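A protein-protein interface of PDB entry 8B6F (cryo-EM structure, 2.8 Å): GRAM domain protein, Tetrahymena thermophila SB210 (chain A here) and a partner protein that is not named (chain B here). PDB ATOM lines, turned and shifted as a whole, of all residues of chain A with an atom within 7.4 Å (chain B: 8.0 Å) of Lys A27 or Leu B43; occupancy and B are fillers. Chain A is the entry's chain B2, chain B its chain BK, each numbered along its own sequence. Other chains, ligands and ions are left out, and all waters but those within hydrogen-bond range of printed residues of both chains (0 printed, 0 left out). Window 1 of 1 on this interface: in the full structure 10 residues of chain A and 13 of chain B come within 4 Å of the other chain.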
ATOM      1  N   ARG A  21      20.766 -37.879 -21.256  1.00  0.00           N
ATOM      2  CA  ARG A  21      20.507 -38.450 -22.574  1.00  0.00           C
ATOM      3  C   ARG A  21      19.852 -37.429 -23.493  1.00  0.00           C
ATOM      4  O   ARG A  21      20.235 -37.296 -24.661  1.00  0.00           O
ATOM      5  CB  ARG A  21      19.618 -39.687 -22.445  1.00  0.00           C
ATOM      6  CG  ARG A  21      20.198 -40.790 -21.577  1.00  0.00           C
ATOM      7  CD  ARG A  21      21.168 -41.663 -22.343  1.00  0.00           C
ATOM      8  NE  ARG A  21      21.645 -42.768 -21.520  1.00  0.00           N
ATOM      9  CZ  ARG A  21      20.993 -43.908 -21.340  1.00  0.00           C
ATOM     10  NH1 ARG A  21      19.826 -44.137 -21.920  1.00  0.00           N
ATOM     11  NH2 ARG A  21      21.521 -44.842 -20.556  1.00  0.00           N
ATOM     12  N   MET A  22      18.861 -36.696 -22.982  1.00  0.00           N
ATOM     13  CA  MET A  22      18.174 -35.701 -23.798  1.00  0.00           C
ATOM     14  C   MET A  22      19.131 -34.607 -24.250  1.00  0.00           C
ATOM     15  O   MET A  22      19.119 -34.203 -25.419  1.00  0.00           O
ATOM     16  CB  MET A  22      17.016 -35.099 -23.006  1.00  0.00           C
ATOM     17  CG  MET A  22      16.226 -34.040 -23.756  1.00  0.00           C
ATOM     18  SD  MET A  22      14.954 -33.270 -22.738  1.00  0.00           S
ATOM     19  CE  MET A  22      15.950 -32.455 -21.492  1.00  0.00           C
ATOM     20  N   LEU A  23      19.968 -34.113 -23.338  1.00  0.00           N
ATOM     21  CA  LEU A  23      20.910 -33.060 -23.699  1.00  0.00           C
ATOM     22  C   LEU A  23      21.929 -33.563 -24.713  1.00  0.00           C
ATOM     23  O   LEU A  23      22.281 -32.846 -25.657  1.00  0.00           O
ATOM     24  CB  LEU A  23      21.605 -32.529 -22.448  1.00  0.00           C
ATOM     25  CG  LEU A  23      22.366 -31.212 -22.606  1.00  0.00           C
ATOM     26  CD1 LEU A  23      21.436 -30.083 -23.022  1.00  0.00           C
ATOM     27  CD2 LEU A  23      23.081 -30.859 -21.318  1.00  0.00           C
ATOM     28  N   GLN A  24      22.417 -34.792 -24.534  1.00  0.00           N
ATOM     29  CA  GLN A  24      23.362 -35.359 -25.490  1.00  0.00           C
ATOM     30  C   GLN A  24      22.734 -35.459 -26.874  1.00  0.00           C
ATOM     31  O   GLN A  24      23.357 -35.097 -27.879  1.00  0.00           O
ATOM     32  CB  GLN A  24      23.821 -36.736 -25.006  1.00  0.00           C
ATOM     33  CG  GLN A  24      25.011 -37.307 -25.762  1.00  0.00           C
ATOM     34  CD  GLN A  24      26.330 -36.725 -25.304  1.00  0.00           C
ATOM     35  OE1 GLN A  24      26.373 -35.869 -24.422  1.00  0.00           O
ATOM     36  NE2 GLN A  24      27.421 -37.191 -25.903  1.00  0.00           N
ATOM     37  N   CYS A  25      21.498 -35.955 -26.947  1.00  0.00           N
ATOM     38  CA  CYS A  25      20.822 -36.066 -28.235  1.00  0.00           C
ATOM     39  C   CYS A  25      20.602 -34.698 -28.866  1.00  0.00           C
ATOM     40  O   CYS A  25      20.816 -34.519 -30.070  1.00  0.00           O
ATOM     41  CB  CYS A  25      19.486 -36.789 -28.072  1.00  0.00           C
ATOM     42  SG  CYS A  25      18.575 -36.980 -29.624  1.00  0.00           S
ATOM     43  N   ALA A  26      20.177 -33.717 -28.068  1.00  0.00           N
ATOM     44  CA  ALA A  26      19.933 -32.385 -28.610  1.00  0.00           C
ATOM     45  C   ALA A  26      21.206 -31.783 -29.187  1.00  0.00           C
ATOM     46  O   ALA A  26      21.181 -31.168 -30.259  1.00  0.00           O
ATOM     47  CB  ALA A  26      19.356 -31.476 -27.525  1.00  0.00           C
ATOM     48  N   LYS A  27      22.328 -31.943 -28.489  1.00  0.00           N
ATOM     49  CA  LYS A  27      23.593 -31.431 -29.004  1.00  0.00           C
ATOM     50  C   LYS A  27      24.001 -32.147 -30.286  1.00  0.00           C
ATOM     51  O   LYS A  27      24.460 -31.510 -31.242  1.00  0.00           O
ATOM     52  CB  LYS A  27      24.681 -31.580 -27.945  1.00  0.00           C
ATOM     53  CG  LYS A  27      24.538 -30.661 -26.749  1.00  0.00           C
ATOM     54  CD  LYS A  27      25.673 -30.894 -25.768  1.00  0.00           C
ATOM     55  CE  LYS A  27      25.608 -29.929 -24.604  1.00  0.00           C
ATOM     56  NZ  LYS A  27      26.748 -30.125 -23.665  1.00  0.00           N
ATOM     57  N   SER A  28      23.846 -33.473 -30.327  1.00  0.00           N
ATOM     58  CA  SER A  28      24.368 -34.242 -31.453  1.00  0.00           C
ATOM     59  C   SER A  28      23.515 -34.060 -32.704  1.00  0.00           C
ATOM     60  O   SER A  28      24.051 -33.938 -33.810  1.00  0.00           O
ATOM     61  CB  SER A  28      24.457 -35.721 -31.077  1.00  0.00           C
ATOM     62  OG  SER A  28      23.183 -36.243 -30.745  1.00  0.00           O
ATOM     63  N   GLU A  29      22.194 -34.047 -32.555  1.00  0.00           N
ATOM     64  CA  GLU A  29      21.312 -34.068 -33.714  1.00  0.00           C
ATOM     65  C   GLU A  29      21.282 -32.714 -34.411  1.00  0.00           C
ATOM     66  O   GLU A  29      21.327 -31.662 -33.768  1.00  0.00           O
ATOM     67  CB  GLU A  29      19.893 -34.455 -33.295  1.00  0.00           C
ATOM     68  CG  GLU A  29      19.772 -35.850 -32.712  1.00  0.00           C
ATOM     69  CD  GLU A  29      20.065 -36.930 -33.727  1.00  0.00           C
ATOM     70  OE1 GLU A  29      20.174 -36.605 -34.928  1.00  0.00           O
ATOM     71  OE2 GLU A  29      20.187 -38.107 -33.327  1.00  0.00           O
ATOM     72  N   ALA A  30      21.201 -32.749 -35.744  1.00  0.00           N
ATOM     73  CA  ALA A  30      20.995 -31.537 -36.527  1.00  0.00           C
ATOM     74  C   ALA A  30      19.551 -31.057 -36.485  1.00  0.00           C
ATOM     75  O   ALA A  30      19.294 -29.882 -36.764  1.00  0.00           O
ATOM     76  CB  ALA A  30      21.409 -31.770 -37.980  1.00  0.00           C
ATOM     77  N   LEU A  31      18.613 -31.938 -36.146  1.00  0.00           N
ATOM     78  CA  LEU A  31      17.200 -31.594 -35.988  1.00  0.00           C
ATOM     79  C   LEU A  31      16.756 -32.087 -34.619  1.00  0.00           C
ATOM     80  O   LEU A  31      15.965 -33.030 -34.504  1.00  0.00           O
ATOM     81  CB  LEU A  31      16.350 -32.214 -37.097  1.00  0.00           C
ATOM     82  CG  LEU A  31      16.720 -31.845 -38.535  1.00  0.00           C
ATOM     83  CD1 LEU A  31      15.858 -32.619 -39.512  1.00  0.00           C
ATOM     84  CD2 LEU A  31      16.579 -30.353 -38.768  1.00  0.00           C
ATOM     85  N   PRO A  32      17.250 -31.462 -33.550  1.00  0.00           N
ATOM     86  CA  PRO A  32      17.003 -32.008 -32.208  1.00  0.00           C
ATOM     87  C   PRO A  32      15.533 -32.119 -31.849  1.00  0.00           C
ATOM     88  O   PRO A  32      15.148 -33.063 -31.151  1.00  0.00           O
ATOM     89  CB  PRO A  32      17.739 -31.019 -31.292  1.00  0.00           C
ATOM     90  CG  PRO A  32      17.829 -29.761 -32.076  1.00  0.00           C
ATOM     91  CD  PRO A  32      17.979 -30.182 -33.503  1.00  0.00           C
ATOM     92  N   ILE A  33      14.697 -31.186 -32.304  1.00  0.00           N
ATOM     93  CA  ILE A  33      13.291 -31.197 -31.908  1.00  0.00           C
ATOM     94  C   ILE A  33      12.605 -32.463 -32.398  1.00  0.00           C
ATOM     95  O   ILE A  33      11.826 -33.087 -31.668  1.00  0.00           O
ATOM     96  CB  ILE A  33      12.579 -29.931 -32.420  1.00  0.00           C
ATOM     97  CG1 ILE A  33      13.162 -28.680 -31.756  1.00  0.00           C
ATOM     98  CG2 ILE A  33      11.074 -30.013 -32.170  1.00  0.00           C
ATOM     99  CD1 ILE A  33      13.110 -28.688 -30.244  1.00  0.00           C
ATOM    100  N   CYS A  36      14.975 -36.096 -31.294  1.00  0.00           N
ATOM    101  CA  CYS A  36      15.185 -36.444 -29.895  1.00  0.00           C
ATOM    102  C   CYS A  36      13.858 -36.642 -29.172  1.00  0.00           C
ATOM    103  O   CYS A  36      13.764 -36.442 -27.960  1.00  0.00           O
ATOM    104  CB  CYS A  36      16.030 -35.385 -29.191  1.00  0.00           C
ATOM    105  SG  CYS A  36      17.665 -35.185 -29.923  1.00  0.00           S
ATOM    106  N   MET B  36      14.800 -20.226 -30.128  1.00  0.00           N
ATOM    107  CA  MET B  36      16.166 -20.734 -29.818  1.00  0.00           C
ATOM    108  C   MET B  36      16.151 -22.249 -29.687  1.00  0.00           C
ATOM    109  O   MET B  36      17.200 -22.880 -29.572  1.00  0.00           O
ATOM    110  CB  MET B  36      16.704 -20.093 -28.538  1.00  0.00           C
ATOM    111  CG  MET B  36      15.846 -20.336 -27.311  1.00  0.00           C
ATOM    112  SD  MET B  36      16.375 -19.374 -25.881  1.00  0.00           S
ATOM    113  CE  MET B  36      18.070 -19.923 -25.698  1.00  0.00           C
ATOM    114  N   GLU B  37      14.951 -22.832 -29.696  1.00  0.00           N
ATOM    115  CA  GLU B  37      14.842 -24.285 -29.653  1.00  0.00           C
ATOM    116  C   GLU B  37      15.437 -24.923 -30.900  1.00  0.00           C
ATOM    117  O   GLU B  37      15.890 -26.071 -30.853  1.00  0.00           O
ATOM    118  CB  GLU B  37      13.380 -24.704 -29.491  1.00  0.00           C
ATOM    119  CG  GLU B  37      12.448 -24.251 -30.613  1.00  0.00           C
ATOM    120  CD  GLU B  37      11.911 -22.848 -30.411  1.00  0.00           C
ATOM    121  OE1 GLU B  37      12.461 -22.116 -29.565  1.00  0.00           O
ATOM    122  OE2 GLU B  37      10.935 -22.479 -31.096  1.00  0.00           O
ATOM    123  N   PHE B  38      15.444 -24.201 -32.019  1.00  0.00           N
ATOM    124  CA  PHE B  38      15.991 -24.703 -33.273  1.00  0.00           C
ATOM    125  C   PHE B  38      17.453 -24.335 -33.474  1.00  0.00           C
ATOM    126  O   PHE B  38      18.035 -24.710 -34.495  1.00  0.00           O
ATOM    127  CB  PHE B  38      15.178 -24.159 -34.453  1.00  0.00           C
ATOM    128  CG  PHE B  38      13.704 -24.410 -34.344  1.00  0.00           C
ATOM    129  CD1 PHE B  38      13.226 -25.627 -33.889  1.00  0.00           C
ATOM    130  CD2 PHE B  38      12.798 -23.425 -34.690  1.00  0.00           C
ATOM    131  CE1 PHE B  38      11.870 -25.857 -33.788  1.00  0.00           C
ATOM    132  CE2 PHE B  38      11.441 -23.649 -34.590  1.00  0.00           C
ATOM    133  CZ  PHE B  38      10.975 -24.869 -34.138  1.00  0.00           C
ATOM    134  N   SER B  39      18.058 -23.618 -32.532  1.00  0.00           N
ATOM    135  CA  SER B  39      19.403 -23.082 -32.700  1.00  0.00           C
ATOM    136  C   SER B  39      20.422 -24.111 -32.224  1.00  0.00           C
ATOM    137  O   SER B  39      20.516 -24.394 -31.027  1.00  0.00           O
ATOM    138  CB  SER B  39      19.551 -21.768 -31.941  1.00  0.00           C
ATOM    139  OG  SER B  39      20.858 -21.250 -32.093  1.00  0.00           O
ATOM    140  N   ASN B  40      21.182 -24.672 -33.165  1.00  0.00           N
ATOM    141  CA  ASN B  40      22.214 -25.638 -32.803  1.00  0.00           C
ATOM    142  C   ASN B  40      23.279 -25.003 -31.919  1.00  0.00           C
ATOM    143  O   ASN B  40      23.755 -25.625 -30.963  1.00  0.00           O
ATOM    144  CB  ASN B  40      22.852 -26.226 -34.061  1.00  0.00           C
ATOM    145  CG  ASN B  40      21.881 -27.061 -34.869  1.00  0.00           C
ATOM    146  OD1 ASN B  40      21.596 -26.756 -36.026  1.00  0.00           O
ATOM    147  ND2 ASN B  40      21.371 -28.125 -34.262  1.00  0.00           N
ATOM    148  N   ALA B  41      23.675 -23.768 -32.228  1.00  0.00           N
ATOM    149  CA  ALA B  41      24.692 -23.097 -31.426  1.00  0.00           C
ATOM    150  C   ALA B  41      24.220 -22.894 -29.993  1.00  0.00           C
ATOM    151  O   ALA B  41      24.948 -23.192 -29.040  1.00  0.00           O
ATOM    152  CB  ALA B  41      25.058 -21.758 -32.065  1.00  0.00           C
ATOM    153  N   LEU B  42      22.996 -22.395 -29.817  1.00  0.00           N
ATOM    154  CA  LEU B  42      22.488 -22.157 -28.470  1.00  0.00           C
ATOM    155  C   LEU B  42      22.291 -23.463 -27.711  1.00  0.00           C
ATOM    156  O   LEU B  42      22.500 -23.516 -26.495  1.00  0.00           O
ATOM    157  CB  LEU B  42      21.185 -21.363 -28.536  1.00  0.00           C
ATOM    158  CG  LEU B  42      21.301 -19.967 -29.153  1.00  0.00           C
ATOM    159  CD1 LEU B  42      19.934 -19.334 -29.320  1.00  0.00           C
ATOM    160  CD2 LEU B  42      22.183 -19.073 -28.304  1.00  0.00           C
ATOM    161  N   LEU B  43      21.887 -24.526 -28.406  1.00  0.00           N
ATOM    162  CA  LEU B  43      21.743 -25.819 -27.746  1.00  0.00           C
ATOM    163  C   LEU B  43      23.094 -26.412 -27.369  1.00  0.00           C
ATOM    164  O   LEU B  43      23.203 -27.095 -26.345  1.00  0.00           O
ATOM    165  CB  LEU B  43      20.966 -26.785 -28.640  1.00  0.00           C
ATOM    166  CG  LEU B  43      19.476 -26.476 -28.806  1.00  0.00           C
ATOM    167  CD1 LEU B  43      18.863 -27.363 -29.870  1.00  0.00           C
ATOM    168  CD2 LEU B  43      18.733 -26.643 -27.489  1.00  0.00           C
ATOM    169  N   SER B  44      24.128 -26.174 -28.177  1.00  0.00           N
ATOM    170  CA  SER B  44      25.455 -26.665 -27.826  1.00  0.00           C
ATOM    171  C   SER B  44      26.066 -25.855 -26.690  1.00  0.00           C
ATOM    172  O   SER B  44      26.907 -26.371 -25.945  1.00  0.00           O
ATOM    173  CB  SER B  44      26.370 -26.637 -29.051  1.00  0.00           C
ATOM    174  OG  SER B  44      26.538 -25.317 -29.535  1.00  0.00           O
ATOM    175  N   GLN B  45      25.672 -24.588 -26.550  1.00  0.00           N
ATOM    176  CA  GLN B  45      26.127 -23.788 -25.422  1.00  0.00           C
ATOM    177  C   GLN B  45      25.595 -24.307 -24.093  1.00  0.00           C
ATOM    178  O   GLN B  45      26.155 -23.975 -23.044  1.00  0.00           O
ATOM    179  CB  GLN B  45      25.715 -22.331 -25.619  1.00  0.00           C
ATOM    180  CG  GLN B  45      26.495 -21.628 -26.716  1.00  0.00           C
ATOM    181  CD  GLN B  45      25.948 -20.251 -27.028  1.00  0.00           C
ATOM    182  OE1 GLN B  45      25.155 -19.699 -26.268  1.00  0.00           O
ATOM    183  NE2 GLN B  45      26.366 -19.692 -28.158  1.00  0.00           N
ATOM    184  N   THR B  46      24.533 -25.109 -24.110  1.00  0.00           N
ATOM    185  CA  THR B  46      24.030 -25.714 -22.887  1.00  0.00           C
ATOM    186  C   THR B  46      24.976 -26.814 -22.413  1.00  0.00           C
ATOM    187  O   THR B  46      25.750 -27.384 -23.185  1.00  0.00           O
ATOM    188  CB  THR B  46      22.629 -26.289 -23.101  1.00  0.00           C
ATOM    189  OG1 THR B  46      22.659 -27.253 -24.162  1.00  0.00           O
ATOM    190  CG2 THR B  46      21.642 -25.186 -23.445  1.00  0.00           C
ATOM    191  N   LYS B  47      24.905 -27.111 -21.118  1.00  0.00           N
ATOM    192  CA  LYS B  47      25.805 -28.086 -20.522  1.00  0.00           C
ATOM    193  C   LYS B  47      25.239 -28.533 -19.183  1.00  0.00           C
ATOM    194  O   LYS B  47      24.363 -27.881 -18.609  1.00  0.00           O
ATOM    195  CB  LYS B  47      27.212 -27.506 -20.345  1.00  0.00           C
ATOM    196  CG  LYS B  47      27.230 -26.179 -19.597  1.00  0.00           C
ATOM    197  CD  LYS B  47      28.607 -25.535 -19.615  1.00  0.00           C
ATOM    198  CE  LYS B  47      29.601 -26.295 -18.762  1.00  0.00           C
ATOM    199  NZ  LYS B  47      29.207 -26.319 -17.326  1.00  0.00           N
ATOM    200  N   LEU B  48      25.754 -29.658 -18.696  1.00  0.00           N
ATOM    201  CA  LEU B  48      25.413 -30.125 -17.366  1.00  0.00           C
ATOM    202  C   LEU B  48      26.073 -29.232 -16.321  1.00  0.00           C
ATOM    203  O   LEU B  48      27.046 -28.534 -16.612  1.00  0.00           O
ATOM    204  CB  LEU B  48      25.857 -31.573 -17.177  1.00  0.00           C
ATOM    205  CG  LEU B  48      25.086 -32.639 -17.959  1.00  0.00           C
ATOM    206  CD1 LEU B  48      25.590 -32.742 -19.389  1.00  0.00           C
ATOM    207  CD2 LEU B  48      25.181 -33.985 -17.263  1.00  0.00           C
ATOM    208  N   GLN B  51      29.732 -30.232 -16.077  1.00  0.00           N
ATOM    209  CA  GLN B  51      30.446 -30.551 -17.304  1.00  0.00           C
ATOM    210  C   GLN B  51      31.443 -29.453 -17.652  1.00  0.00           C
ATOM    211  O   GLN B  51      31.178 -28.265 -17.451  1.00  0.00           O
ATOM    212  CB  GLN B  51      29.458 -30.747 -18.454  1.00  0.00           C
ATOM    213  CG  GLN B  51      30.106 -31.152 -19.764  1.00  0.00           C
ATOM    214  CD  GLN B  51      29.087 -31.485 -20.832  1.00  0.00           C
ATOM    215  OE1 GLN B  51      27.898 -31.214 -20.678  1.00  0.00           O
ATOM    216  NE2 GLN B  51      29.550 -32.080 -21.925  1.00  0.00           N
ATOM    217  N   TYR B  53      34.916 -28.669 -20.661  1.00  0.00           N
ATOM    218  CA  TYR B  53      35.530 -29.065 -21.920  1.00  0.00           C
ATOM    219  C   TYR B  53      37.036 -28.869 -21.842  1.00  0.00           C
ATOM    220  O   TYR B  53      37.505 -27.794 -21.453  1.00  0.00           O
ATOM    221  CB  TYR B  53      34.958 -28.257 -23.088  1.00  0.00           C
ATOM    222  CG  TYR B  53      33.452 -28.304 -23.180  1.00  0.00           C
ATOM    223  CD1 TYR B  53      32.802 -29.428 -23.670  1.00  0.00           C
ATOM    224  CD2 TYR B  53      32.680 -27.224 -22.777  1.00  0.00           C
ATOM    225  CE1 TYR B  53      31.425 -29.476 -23.756  1.00  0.00           C
ATOM    226  CE2 TYR B  53      31.303 -27.262 -22.858  1.00  0.00           C
ATOM    227  CZ  TYR B  53      30.682 -28.391 -23.348  1.00  0.00           C
ATOM    228  OH  TYR B  53      29.311 -28.434 -23.432  1.00  0.00           O
ATOM    229  N   ASP B  94      33.429 -33.034 -27.555  1.00  0.00           N
ATOM    230  CA  ASP B  94      32.026 -33.169 -27.205  1.00  0.00           C
ATOM    231  C   ASP B  94      31.157 -33.164 -28.460  1.00  0.00           C
ATOM    232  O   ASP B  94      31.583 -32.763 -29.545  1.00  0.00           O
ATOM    233  CB  ASP B  94      31.607 -32.035 -26.266  1.00  0.00           C
ATOM    234  CG  ASP B  94      30.237 -32.256 -25.657  1.00  0.00           C
ATOM    235  OD1 ASP B  94      30.083 -33.200 -24.856  1.00  0.00           O
ATOM    236  OD2 ASP B  94      29.313 -31.480 -25.978  1.00  0.00           O
ATOM    237  N   VAL B  95      29.911 -33.612 -28.292  1.00  0.00           N
ATOM    238  CA  VAL B  95      29.011 -33.753 -29.433  1.00  0.00           C
ATOM    239  C   VAL B  95      28.747 -32.400 -30.081  1.00  0.00           C
ATOM    240  O   VAL B  95      28.734 -32.279 -31.312  1.00  0.00           O
ATOM    241  CB  VAL B  95      27.699 -34.442 -29.011  1.00  0.00           C
ATOM    242  CG1 VAL B  95      27.927 -35.924 -28.807  1.00  0.00           C
ATOM    243  CG2 VAL B  95      27.131 -33.812 -27.746  1.00  0.00           C
ATOM    244  N   GLY B  96      28.524 -31.364 -29.272  1.00  0.00           N
ATOM    245  CA  GLY B  96      28.275 -30.048 -29.837  1.00  0.00           C
ATOM    246  C   GLY B  96      29.476 -29.505 -30.584  1.00  0.00           C
ATOM    247  O   GLY B  96      29.339 -28.929 -31.665  1.00  0.00           O
ATOM    248  N   ILE B  97      30.670 -29.673 -30.016  1.00  0.00           N
ATOM    249  CA  ILE B  97      31.886 -29.231 -30.692  1.00  0.00           C
ATOM    250  C   ILE B  97      32.052 -29.968 -32.013  1.00  0.00           C
ATOM    251  O   ILE B  97      32.399 -29.369 -33.038  1.00  0.00           O
ATOM    252  CB  ILE B  97      33.106 -29.422 -29.773  1.00  0.00           C
ATOM    253  CG1 ILE B  97      32.982 -28.515 -28.546  1.00  0.00           C
ATOM    254  CG2 ILE B  97      34.405 -29.147 -30.531  1.00  0.00           C
ATOM    255  CD1 ILE B  97      34.013 -28.777 -27.476  1.00  0.00           C
ATOM    256  N   ARG B  98      31.806 -31.278 -32.011  1.00  0.00           N
ATOM    257  CA  ARG B  98      31.920 -32.055 -33.240  1.00  0.00           C
ATOM    258  C   ARG B  98      30.913 -31.591 -34.285  1.00  0.00           C
ATOM    259  O   ARG B  98      31.243 -31.487 -35.470  1.00  0.00           O
ATOM    260  CB  ARG B  98      31.734 -33.540 -32.939  1.00  0.00           C
ATOM    261  CG  ARG B  98      32.868 -34.151 -32.134  1.00  0.00           C
ATOM    262  CD  ARG B  98      32.689 -35.650 -31.987  1.00  0.00           C
ATOM    263  NE  ARG B  98      31.848 -35.986 -30.845  1.00  0.00           N
ATOM    264  CZ  ARG B  98      31.278 -37.167 -30.656  1.00  0.00           C
ATOM    265  NH1 ARG B  98      31.392 -38.141 -31.541  1.00  0.00           N
ATOM    266  NH2 ARG B  98      30.568 -37.374 -29.551  1.00  0.00           N
ATOM    267  N   ARG B  99      29.680 -31.303 -33.864  1.00  0.00           N
ATOM    268  CA  ARG B  99      28.676 -30.825 -34.810  1.00  0.00           C
ATOM    269  C   ARG B  99      29.114 -29.512 -35.442  1.00  0.00           C
ATOM    270  O   ARG B  99      29.025 -29.335 -36.663  1.00  0.00           O
ATOM    271  CB  ARG B  99      27.332 -30.656 -34.103  1.00  0.00           C
ATOM    272  CG  ARG B  99      26.165 -30.447 -35.051  1.00  0.00           C
ATOM    273  CD  ARG B  99      25.712 -31.768 -35.652  1.00  0.00           C
ATOM    274  NE  ARG B  99      25.024 -31.588 -36.925  1.00  0.00           N
ATOM    275  CZ  ARG B  99      25.610 -31.637 -38.114  1.00  0.00           C
ATOM    276  NH1 ARG B  99      26.907 -31.867 -38.239  1.00  0.00           N
ATOM    277  NH2 ARG B  99      24.875 -31.450 -39.206  1.00  0.00           N
ATOM    278  N   TYR B 100      29.585 -28.572 -34.623  1.00  0.00           N
ATOM    279  CA  TYR B 100      30.057 -27.300 -35.157  1.00  0.00           C
ATOM    280  C   TYR B 100      31.223 -27.508 -36.114  1.00  0.00           C
ATOM    281  O   TYR B 100      31.285 -26.881 -37.177  1.00  0.00           O
ATOM    282  CB  TYR B 100      30.465 -26.374 -34.014  1.00  0.00           C
ATOM    283  CG  TYR B 100      31.094 -25.083 -34.478  1.00  0.00           C
ATOM    284  CD1 TYR B 100      30.314 -23.974 -34.767  1.00  0.00           C
ATOM    285  CD2 TYR B 100      32.470 -24.972 -34.623  1.00  0.00           C
ATOM    286  CE1 TYR B 100      30.884 -22.793 -35.190  1.00  0.00           C
ATOM    287  CE2 TYR B 100      33.050 -23.796 -35.046  1.00  0.00           C
ATOM    288  CZ  TYR B 100      32.251 -22.709 -35.327  1.00  0.00           C
ATOM    289  OH  TYR B 100      32.824 -21.533 -35.749  1.00  0.00           O
ATOM    290  N   ASP B 103      29.955 -28.938 -39.481  1.00  0.00           N
ATOM    291  CA  ASP B 103      29.269 -27.917 -40.265  1.00  0.00           C
ATOM    292  C   ASP B 103      30.265 -26.936 -40.868  1.00  0.00           C
ATOM    293  O   ASP B 103      30.145 -26.556 -42.038  1.00  0.00           O
ATOM    294  CB  ASP B 103      28.254 -27.179 -39.394  1.00  0.00           C
ATOM    295  CG  ASP B 103      27.153 -28.086 -38.891  1.00  0.00           C
ATOM    296  OD1 ASP B 103      26.811 -29.056 -39.601  1.00  0.00           O
ATOM    297  OD2 ASP B 103      26.625 -27.831 -37.789  1.00  0.00           O
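Among the printed residues, pairs that only touch across the chains: Leu A23 with Thr B46 (3.3 Å), Leu A23 with Lys B47 (3.8 Å), Leu A23 with Leu B48 (3.7 Å), Gln A24 with Val B95 (3.2 Å), Lys A27 with Leu B43 (3.8 Å), Lys A27 with Lys B47 (3.9 Å), Lys A27 with Val B95 (3.3 Å), Ser A28 with Arg B99 (3.3 Å), Glu A29 with Asn B40 (3.6 Å), Ala A30 with Asn B40 (3.7 Å), Ala A30 with Arg B99 (3.7 Å), Pro A32 with Leu B43 (3.4 Å), Ile A33 with Glu B37 (3.9 Å) and Ile A33 with Phe B38 (3.7 Å).
The backbone carbonyl oxygen of Thr B46 sits close to the side-chain amino group of Lys A27, at 3.0 Å. The side-chain amide oxygen (OE1) of Gln B51 sits at hydrogen-bond distance from the side-chain amino group (NZ) of Lys A27 (3.4 Å). The side-chain amino group of Lys A27 is in hydrogen-bond range of the side-chain hydroxyl of Tyr B53 (3.1 Å). The side-chain amino group (NZ) of Lys A27 is in salt-bridge range of the side-chain carboxylate (OD2) of Asp B94, 3.7 Å away.
Of the printed residues of chain B, Leu A23 touches Thr B46, Lys B47 and Leu B48. No residue of chain B comes within 4 Å of Ala A26. Of the printed residues of chain B, Lys A27 touches Leu B43, Thr B46, Lys B47, Gln B51, Tyr B53, Asp B94 and Val B95. Of the printed residues of chain B, Glu A29 touches Asn B40 (3.6 Å). Printed residues of chain B within 4 Å of Pro A32: Leu B43. Cys A36 touches none of the printed residues of chain B. Leu B43 touches just these residues of chain A: Lys A27 (3.8 Å) and Pro A32 (3.4 Å). Printed residues of chain A within 4 Å of Asp B94: Lys A27. Of the printed residues of chain A, Arg B99 touches Ser A28 and Ala A30.
The backbone carbonyl oxygen (O) of Asn B40 is in hydrogen-bond range of the side-chain hydroxyl (OG) of Ser B44, 3.1 Å away. O of Gln B51 sits at hydrogen-bond distance from NZ of Lys B47 (2.8 Å). The side-chain amide oxygen of Gln B51 sits close to the backbone NH of Leu B48 (3.3 Å). NE2 of Gln B51 is in hydrogen-bond range of OD1 of Asp B94 (3.2 Å). The backbone NH (N) of Gly B96 lies close to the side-chain carboxylate (OD2) of Asp B94 (3.4 Å). The side-chain sulfur of Cys A25 forms a disulfide with the side-chain sulfur of Cys A36, at 2.0 Å.
Of the 23 printed residues of chain B, 12 touch a printed residue of chain A. Printed residues of chain B that touch a printed residue of chain A: Glu B37, Phe B38, Asn B40, Leu B43, Thr B46, Lys B47, Leu B48, Gln B51, Tyr B53, Asp B94, Val B95 and Arg B99. Hydrophobic or aromatic side chains of chain B that line the printed part of chain A: Phe B38, Leu B43, Leu B48, Tyr B53 and Val B95. Printed residues of chain A that touch a printed residue of chain B: Leu A23, Gln A24, Lys A27, Ser A28, Glu A29, Ala A30, Pro A32 and Ile A33. Hydrophobic or aromatic side chains of chain A that line the printed part of chain B: Leu A23, Ala A30, Pro A32 and Ile A33.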
